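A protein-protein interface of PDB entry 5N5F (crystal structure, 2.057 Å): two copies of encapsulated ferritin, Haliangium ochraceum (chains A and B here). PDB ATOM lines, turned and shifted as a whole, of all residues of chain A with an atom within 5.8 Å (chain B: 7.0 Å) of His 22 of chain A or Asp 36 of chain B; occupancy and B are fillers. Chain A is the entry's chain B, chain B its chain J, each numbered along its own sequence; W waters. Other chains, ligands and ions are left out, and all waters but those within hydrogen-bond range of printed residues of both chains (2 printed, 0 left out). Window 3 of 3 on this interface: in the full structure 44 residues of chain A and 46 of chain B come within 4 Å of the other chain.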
ATOM      1  N   GLN A   6      32.134 -24.132  15.458  1.00  0.00           N
ATOM      2  CA  GLN A   6      30.963 -23.360  15.060  1.00  0.00           C
ATOM      3  C   GLN A   6      29.697 -24.201  15.221  1.00  0.00           C
ATOM      4  O   GLN A   6      28.642 -23.679  15.580  1.00  0.00           O
ATOM      5  CB  GLN A   6      31.110 -22.872  13.613  1.00  0.00           C
ATOM      6  CG  GLN A   6      29.946 -22.036  13.094  1.00  0.00           C
ATOM      7  CD  GLN A   6      29.822 -20.690  13.781  1.00  0.00           C
ATOM      8  OE1 GLN A   6      30.464 -20.435  14.799  1.00  0.00           O
ATOM      9  NE2 GLN A   6      28.986 -19.820  13.226  1.00  0.00           N
ATOM     10  N   LEU A   7      29.809 -25.500  14.959  1.00  0.00           N
ATOM     11  CA  LEU A   7      28.694 -26.412  15.170  1.00  0.00           C
ATOM     12  C   LEU A   7      28.349 -26.498  16.653  1.00  0.00           C
ATOM     13  O   LEU A   7      29.220 -26.404  17.523  1.00  0.00           O
ATOM     14  CB  LEU A   7      29.031 -27.806  14.641  1.00  0.00           C
ATOM     15  CG  LEU A   7      29.194 -27.958  13.129  1.00  0.00           C
ATOM     16  CD1 LEU A   7      29.835 -29.297  12.802  1.00  0.00           C
ATOM     17  CD2 LEU A   7      27.851 -27.826  12.429  1.00  0.00           C
ATOM     18  N   GLU A  17      24.547 -34.007   5.038  1.00  0.00           N
ATOM     19  CA  GLU A  17      23.723 -32.965   4.434  1.00  0.00           C
ATOM     20  C   GLU A  17      23.507 -31.812   5.404  1.00  0.00           C
ATOM     21  O   GLU A  17      23.545 -30.641   5.006  1.00  0.00           O
ATOM     22  CB  GLU A  17      22.384 -33.546   3.981  1.00  0.00           C
ATOM     23  CG  GLU A  17      22.492 -34.529   2.820  1.00  0.00           C
ATOM     24  CD  GLU A  17      23.115 -35.855   3.218  1.00  0.00           C
ATOM     25  OE1 GLU A  17      22.947 -36.269   4.385  1.00  0.00           O
ATOM     26  OE2 GLU A  17      23.780 -36.479   2.365  1.00  0.00           O
ATOM     27  N   THR A  18      23.282 -32.120   6.683  1.00  0.00           N
ATOM     28  CA  THR A  18      23.157 -31.068   7.684  1.00  0.00           C
ATOM     29  C   THR A  18      24.425 -30.229   7.753  1.00  0.00           C
ATOM     30  O   THR A  18      24.360 -28.996   7.834  1.00  0.00           O
ATOM     31  CB  THR A  18      22.845 -31.679   9.050  1.00  0.00           C
ATOM     32  OG1 THR A  18      21.585 -32.361   8.993  1.00  0.00           O
ATOM     33  CG2 THR A  18      22.776 -30.605  10.129  1.00  0.00           C
ATOM     34  N   LYS A  19      25.591 -30.878   7.715  1.00  0.00           N
ATOM     35  CA  LYS A  19      26.846 -30.143   7.833  1.00  0.00           C
ATOM     36  C   LYS A  19      27.107 -29.285   6.601  1.00  0.00           C
ATOM     37  O   LYS A  19      27.595 -28.156   6.719  1.00  0.00           O
ATOM     38  CB  LYS A  19      27.999 -31.117   8.072  1.00  0.00           C
ATOM     39  CG  LYS A  19      27.870 -31.901   9.373  1.00  0.00           C
ATOM     40  CD  LYS A  19      29.220 -32.383   9.880  1.00  0.00           C
ATOM     41  CE  LYS A  19      29.743 -33.559   9.075  1.00  0.00           C
ATOM     42  NZ  LYS A  19      29.254 -34.854   9.613  1.00  0.00           N
ATOM     43  N   ASN A  20      26.785 -29.796   5.410  1.00  0.00           N
ATOM     44  CA  ASN A  20      26.924 -28.981   4.207  1.00  0.00           C
ATOM     45  C   ASN A  20      25.912 -27.844   4.189  1.00  0.00           C
ATOM     46  O   ASN A  20      26.216 -26.754   3.693  1.00  0.00           O
ATOM     47  CB  ASN A  20      26.773 -29.851   2.960  1.00  0.00           C
ATOM     48  CG  ASN A  20      27.966 -30.757   2.737  1.00  0.00           C
ATOM     49  OD1 ASN A  20      29.113 -30.354   2.937  1.00  0.00           O
ATOM     50  ND2 ASN A  20      27.702 -31.991   2.326  1.00  0.00           N
ATOM     51  N   MET A  21      24.711 -28.078   4.718  1.00  0.00           N
ATOM     52  CA  MET A  21      23.742 -26.996   4.855  1.00  0.00           C
ATOM     53  C   MET A  21      24.230 -25.952   5.851  1.00  0.00           C
ATOM     54  O   MET A  21      23.997 -24.751   5.670  1.00  0.00           O
ATOM     55  CB  MET A  21      22.393 -27.561   5.295  1.00  0.00           C
ATOM     56  CG  MET A  21      21.232 -26.595   5.158  1.00  0.00           C
ATOM     57  SD  MET A  21      20.922 -26.049   3.465  1.00  0.00           S
ATOM     58  CE  MET A  21      20.913 -27.596   2.566  1.00  0.00           C
ATOM     59  N   HIS A  22      24.898 -26.393   6.918  1.00  0.00           N
ATOM     60  CA  HIS A  22      25.490 -25.455   7.866  1.00  0.00           C
ATOM     61  C   HIS A  22      26.508 -24.556   7.173  1.00  0.00           C
ATOM     62  O   HIS A  22      26.459 -23.327   7.301  1.00  0.00           O
ATOM     63  CB  HIS A  22      26.131 -26.230   9.020  1.00  0.00           C
ATOM     64  CG  HIS A  22      27.107 -25.428   9.825  1.00  0.00           C
ATOM     65  ND1 HIS A  22      26.721 -24.387  10.642  1.00  0.00           N
ATOM     66  CD2 HIS A  22      28.455 -25.516   9.939  1.00  0.00           C
ATOM     67  CE1 HIS A  22      27.788 -23.869  11.224  1.00  0.00           C
ATOM     68  NE2 HIS A  22      28.853 -24.535  10.814  1.00  0.00           N
ATOM     69  N   ARG A  23      27.432 -25.155   6.417  1.00  0.00           N
ATOM     70  CA  ARG A  23      28.434 -24.364   5.710  1.00  0.00           C
ATOM     71  C   ARG A  23      27.780 -23.345   4.786  1.00  0.00           C
ATOM     72  O   ARG A  23      28.230 -22.198   4.696  1.00  0.00           O
ATOM     73  CB  ARG A  23      29.371 -25.283   4.924  1.00  0.00           C
ATOM     74  CG  ARG A  23      30.183 -26.219   5.803  1.00  0.00           C
ATOM     75  CD  ARG A  23      31.138 -27.088   4.999  1.00  0.00           C
ATOM     76  NE  ARG A  23      31.939 -27.941   5.873  1.00  0.00           N
ATOM     77  CZ  ARG A  23      31.657 -29.205   6.184  1.00  0.00           C
ATOM     78  NH1 ARG A  23      30.588 -29.808   5.687  1.00  0.00           N
ATOM     79  NH2 ARG A  23      32.462 -29.875   6.999  1.00  0.00           N
ATOM     80  N   ALA A  24      26.706 -23.738   4.100  1.00  0.00           N
ATOM     81  CA  ALA A  24      26.047 -22.808   3.190  1.00  0.00           C
ATOM     82  C   ALA A  24      25.296 -21.725   3.954  1.00  0.00           C
ATOM     83  O   ALA A  24      25.339 -20.549   3.574  1.00  0.00           O
ATOM     84  CB  ALA A  24      25.102 -23.566   2.259  1.00  0.00           C
ATOM     85  N   LEU A  25      24.606 -22.094   5.035  1.00  0.00           N
ATOM     86  CA  LEU A  25      23.841 -21.106   5.791  1.00  0.00           C
ATOM     87  C   LEU A  25      24.754 -20.071   6.445  1.00  0.00           C
ATOM     88  O   LEU A  25      24.422 -18.880   6.480  1.00  0.00           O
ATOM     89  CB  LEU A  25      22.968 -21.806   6.838  1.00  0.00           C
ATOM     90  CG  LEU A  25      21.717 -22.502   6.287  1.00  0.00           C
ATOM     91  CD1 LEU A  25      21.050 -23.383   7.349  1.00  0.00           C
ATOM     92  CD2 LEU A  25      20.729 -21.473   5.763  1.00  0.00           C
ATOM     93  N   VAL A  26      25.906 -20.488   6.970  1.00  0.00           N
ATOM     94  CA  VAL A  26      26.801 -19.499   7.565  1.00  0.00           C
ATOM     95  C   VAL A  26      27.364 -18.582   6.490  1.00  0.00           C
ATOM     96  O   VAL A  26      27.574 -17.386   6.732  1.00  0.00           O
ATOM     97  CB  VAL A  26      27.921 -20.175   8.380  1.00  0.00           C
ATOM     98  CG1 VAL A  26      27.326 -21.003   9.510  1.00  0.00           C
ATOM     99  CG2 VAL A  26      28.822 -21.028   7.493  1.00  0.00           C
ATOM    100  N   THR A  27      27.597 -19.111   5.284  1.00  0.00           N
ATOM    101  CA  THR A  27      28.098 -18.277   4.197  1.00  0.00           C
ATOM    102  C   THR A  27      27.049 -17.260   3.769  1.00  0.00           C
ATOM    103  O   THR A  27      27.351 -16.070   3.608  1.00  0.00           O
ATOM    104  CB  THR A  27      28.521 -19.150   3.014  1.00  0.00           C
ATOM    105  OG1 THR A  27      29.525 -20.082   3.437  1.00  0.00           O
ATOM    106  CG2 THR A  27      29.085 -18.294   1.881  1.00  0.00           C
ATOM    107  N   GLU B  31      16.839 -15.476  11.595  1.00  0.00           N
ATOM    108  CA  GLU B  31      15.982 -16.583  11.195  1.00  0.00           C
ATOM    109  C   GLU B  31      16.789 -17.683  10.515  1.00  0.00           C
ATOM    110  O   GLU B  31      16.594 -18.868  10.804  1.00  0.00           O
ATOM    111  CB  GLU B  31      14.863 -16.054  10.298  1.00  0.00           C
ATOM    112  CG  GLU B  31      13.891 -15.166  11.073  1.00  0.00           C
ATOM    113  CD  GLU B  31      13.038 -14.266  10.196  1.00  0.00           C
ATOM    114  OE1 GLU B  31      13.390 -14.054   9.018  1.00  0.00           O
ATOM    115  OE2 GLU B  31      12.015 -13.757  10.700  1.00  0.00           O
ATOM    116  N   LEU B  32      17.716 -17.314   9.628  1.00  0.00           N
ATOM    117  CA  LEU B  32      18.596 -18.316   9.035  1.00  0.00           C
ATOM    118  C   LEU B  32      19.469 -18.982  10.091  1.00  0.00           C
ATOM    119  O   LEU B  32      19.788 -20.171   9.974  1.00  0.00           O
ATOM    120  CB  LEU B  32      19.465 -17.677   7.948  1.00  0.00           C
ATOM    121  CG  LEU B  32      18.705 -17.096   6.752  1.00  0.00           C
ATOM    122  CD1 LEU B  32      19.656 -16.293   5.870  1.00  0.00           C
ATOM    123  CD2 LEU B  32      18.029 -18.197   5.950  1.00  0.00           C
ATOM    124  N   GLU B  33      19.857 -18.245  11.131  1.00  0.00           N
ATOM    125  CA  GLU B  33      20.636 -18.849  12.207  1.00  0.00           C
ATOM    126  C   GLU B  33      19.828 -19.904  12.951  1.00  0.00           C
ATOM    127  O   GLU B  33      20.361 -20.963  13.308  1.00  0.00           O
ATOM    128  CB  GLU B  33      21.126 -17.770  13.173  1.00  0.00           C
ATOM    129  CG  GLU B  33      22.270 -16.934  12.620  1.00  0.00           C
ATOM    130  CD  GLU B  33      22.791 -15.915  13.616  1.00  0.00           C
ATOM    131  OE1 GLU B  33      21.998 -15.415  14.443  1.00  0.00           O
ATOM    132  OE2 GLU B  33      24.002 -15.619  13.569  1.00  0.00           O
ATOM    133  N   ALA B  34      18.543 -19.634  13.196  1.00  0.00           N
ATOM    134  CA  ALA B  34      17.700 -20.621  13.861  1.00  0.00           C
ATOM    135  C   ALA B  34      17.462 -21.840  12.981  1.00  0.00           C
ATOM    136  O   ALA B  34      17.361 -22.960  13.493  1.00  0.00           O
ATOM    137  CB  ALA B  34      16.367 -19.990  14.264  1.00  0.00           C
ATOM    138  N   VAL B  35      17.368 -21.644  11.662  1.00  0.00           N
ATOM    139  CA  VAL B  35      17.227 -22.773  10.746  1.00  0.00           C
ATOM    140  C   VAL B  35      18.411 -23.719  10.893  1.00  0.00           C
ATOM    141  O   VAL B  35      18.249 -24.941  10.970  1.00  0.00           O
ATOM    142  CB  VAL B  35      17.081 -22.271   9.296  1.00  0.00           C
ATOM    143  CG1 VAL B  35      17.201 -23.421   8.301  1.00  0.00           C
ATOM    144  CG2 VAL B  35      15.743 -21.561   9.114  1.00  0.00           C
ATOM    145  N   ASP B  36      19.624 -23.167  10.919  1.00  0.00           N
ATOM    146  CA  ASP B  36      20.808 -24.001  11.089  1.00  0.00           C
ATOM    147  C   ASP B  36      20.787 -24.700  12.443  1.00  0.00           C
ATOM    148  O   ASP B  36      20.931 -25.927  12.527  1.00  0.00           O
ATOM    149  CB  ASP B  36      22.066 -23.141  10.930  1.00  0.00           C
ATOM    150  CG  ASP B  36      23.341 -23.964  10.847  1.00  0.00           C
ATOM    151  OD1 ASP B  36      23.255 -25.190  10.619  1.00  0.00           O
ATOM    152  OD2 ASP B  36      24.435 -23.376  10.999  1.00  0.00           O
ATOM    153  N   TRP B  37      20.566 -23.936  13.516  1.00  0.00           N
ATOM    154  CA  TRP B  37      20.685 -24.483  14.864  1.00  0.00           C
ATOM    155  C   TRP B  37      19.622 -25.539  15.140  1.00  0.00           C
ATOM    156  O   TRP B  37      19.913 -26.569  15.759  1.00  0.00           O
ATOM    157  CB  TRP B  37      20.599 -23.354  15.890  1.00  0.00           C
ATOM    158  CG  TRP B  37      21.670 -22.312  15.706  1.00  0.00           C
ATOM    159  CD1 TRP B  37      22.832 -22.446  15.001  1.00  0.00           C
ATOM    160  CD2 TRP B  37      21.668 -20.976  16.224  1.00  0.00           C
ATOM    161  NE1 TRP B  37      23.556 -21.278  15.053  1.00  0.00           N
ATOM    162  CE2 TRP B  37      22.864 -20.360  15.799  1.00  0.00           C
ATOM    163  CE3 TRP B  37      20.772 -20.241  17.009  1.00  0.00           C
ATOM    164  CZ2 TRP B  37      23.186 -19.046  16.132  1.00  0.00           C
ATOM    165  CZ3 TRP B  37      21.095 -18.938  17.340  1.00  0.00           C
ATOM    166  CH2 TRP B  37      22.290 -18.353  16.902  1.00  0.00           C
ATOM    167  N   TYR B  38      18.384 -25.301  14.698  1.00  0.00           N
ATOM    168  CA  TYR B  38      17.321 -26.271  14.948  1.00  0.00           C
ATOM    169  C   TYR B  38      17.584 -27.580  14.215  1.00  0.00           C
ATOM    170  O   TYR B  38      17.339 -28.662  14.764  1.00  0.00           O
ATOM    171  CB  TYR B  38      15.962 -25.695  14.544  1.00  0.00           C
ATOM    172  CG  TYR B  38      15.463 -24.554  15.412  1.00  0.00           C
ATOM    173  CD1 TYR B  38      16.295 -23.923  16.333  1.00  0.00           C
ATOM    174  CD2 TYR B  38      14.154 -24.115  15.314  1.00  0.00           C
ATOM    175  CE1 TYR B  38      15.831 -22.882  17.121  1.00  0.00           C
ATOM    176  CE2 TYR B  38      13.680 -23.080  16.097  1.00  0.00           C
ATOM    177  CZ  TYR B  38      14.522 -22.467  16.998  1.00  0.00           C
ATOM    178  OH  TYR B  38      14.048 -21.436  17.776  1.00  0.00           O
ATOM    179  N   GLN B  39      18.078 -27.509  12.974  1.00  0.00           N
ATOM    180  CA  GLN B  39      18.369 -28.732  12.229  1.00  0.00           C
ATOM    181  C   GLN B  39      19.482 -29.526  12.899  1.00  0.00           C
ATOM    182  O   GLN B  39      19.446 -30.762  12.930  1.00  0.00           O
ATOM    183  CB  GLN B  39      18.751 -28.402  10.785  1.00  0.00           C
ATOM    184  CG  GLN B  39      19.019 -29.630   9.913  1.00  0.00           C
ATOM    185  CD  GLN B  39      17.786 -30.499   9.733  1.00  0.00           C
ATOM    186  OE1 GLN B  39      16.804 -30.075   9.127  1.00  0.00           O
ATOM    187  NE2 GLN B  39      17.827 -31.715  10.270  1.00  0.00           N
ATOM    188  N   GLN B  40      20.489 -28.833  13.432  1.00  0.00           N
ATOM    189  CA  GLN B  40      21.553 -29.520  14.150  1.00  0.00           C
ATOM    190  C   GLN B  40      21.012 -30.225  15.385  1.00  0.00           C
ATOM    191  O   GLN B  40      21.367 -31.376  15.659  1.00  0.00           O
ATOM    192  CB  GLN B  40      22.645 -28.527  14.544  1.00  0.00           C
ATOM    193  CG  GLN B  40      23.429 -27.958  13.380  1.00  0.00           C
ATOM    194  CD  GLN B  40      24.594 -27.109  13.845  1.00  0.00           C
ATOM    195  OE1 GLN B  40      25.280 -27.456  14.803  1.00  0.00           O
ATOM    196  NE2 GLN B  40      24.809 -25.982  13.181  1.00  0.00           N
ATOM    197  N   ARG B  41      20.142 -29.549  16.141  1.00  0.00           N
ATOM    198  CA  ARG B  41      19.632 -30.134  17.375  1.00  0.00           C
ATOM    199  C   ARG B  41      18.692 -31.299  17.100  1.00  0.00           C
ATOM    200  O   ARG B  41      18.666 -32.265  17.870  1.00  0.00           O
ATOM    201  CB  ARG B  41      18.941 -29.059  18.214  1.00  0.00           C
ATOM    202  CG  ARG B  41      19.921 -28.023  18.755  1.00  0.00           C
ATOM    203  CD  ARG B  41      19.376 -27.279  19.961  1.00  0.00           C
ATOM    204  NE  ARG B  41      18.595 -26.102  19.591  1.00  0.00           N
ATOM    205  CZ  ARG B  41      19.090 -24.874  19.456  1.00  0.00           C
ATOM    206  NH1 ARG B  41      20.380 -24.635  19.651  1.00  0.00           N
ATOM    207  NH2 ARG B  41      18.284 -23.875  19.117  1.00  0.00           N
ATOM    208  N   LYS B  58      11.584 -25.182  12.861  1.00  0.00           N
ATOM    209  CA  LYS B  58      12.596 -24.863  11.856  1.00  0.00           C
ATOM    210  C   LYS B  58      11.940 -24.440  10.552  1.00  0.00           C
ATOM    211  O   LYS B  58      12.318 -23.433   9.944  1.00  0.00           O
ATOM    212  CB  LYS B  58      13.505 -26.071  11.611  1.00  0.00           C
ATOM    213  CG  LYS B  58      14.472 -25.920  10.427  1.00  0.00           C
ATOM    214  CD  LYS B  58      14.794 -27.253   9.782  1.00  0.00           C
ATOM    215  CE  LYS B  58      15.683 -27.067   8.565  1.00  0.00           C
ATOM    216  NZ  LYS B  58      15.728 -28.289   7.712  1.00  0.00           N
HETATM  217  O   HOH W   1      22.503 -27.278   9.166  1.00  0.00           O
HETATM  218  O   HOH W   2      26.329 -23.792  14.330  1.00  0.00           O
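OD2 of Asp 36 of chain B is in hydrogen-bond range of ND1 of His 22 of chain A, 2.5 Å away.
OE1 of Gln 39 of chain B sits at hydrogen-bond distance from NZ of Lys 58 of chain B (2.5 Å). The side-chain carboxylate of Asp 36 of chain B lies within hydrogen-bond range of the side-chain amide nitrogen of Gln 40 of chain B (3.1 Å).
Gln 40 of chain B touches Leu 7 of chain A. Thr 18 of chain A touches Gln 39 of chain B. ND1 of His 22 of chain A touches NE2 of Gln 40 of chain B, at 3.6 Å. Leu 25 of chain A touches Val 35 of chain B. Leu 25 of chain A touches Asp 36 of chain B.
Of chain B, only Asp 36 and Gln 40 come within 4 Å of His 22 of chain A. Of the printed residues of chain A, Val 35 of chain B touches Leu 25. Tyr 38 of chain B touches none of the printed residues of chain A. Of the printed residues of chain A, Gln 39 of chain B touches Thr 18. Of the printed residues of chain A, Gln 40 of chain B touches Leu 7 and His 22. The nearest residue of chain A that does not touch Asp 36 of chain B is Val 26 of chain A (4.03 Å).
Hydrophobic or aromatic side chains of chain B within 4 Å of the printed part of chain A: Val 35. Of the 13 printed residues of chain A, 4 touch a printed residue of chain B. Among the printed residues, 6 pairs touch across the chains.
No position is printed for both chains.
Water W2 bridges O of Gln 6 of chain A (2.6 Å) and NE2 of Gln 40 of chain B (2.9 Å). Water W1 lies within hydrogen-bond range of OD1 of Asp 36 of chain B (2.7 Å), O of Thr 18 of chain A (2.9 Å) and N of His 22 of chain A (3.4 Å).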
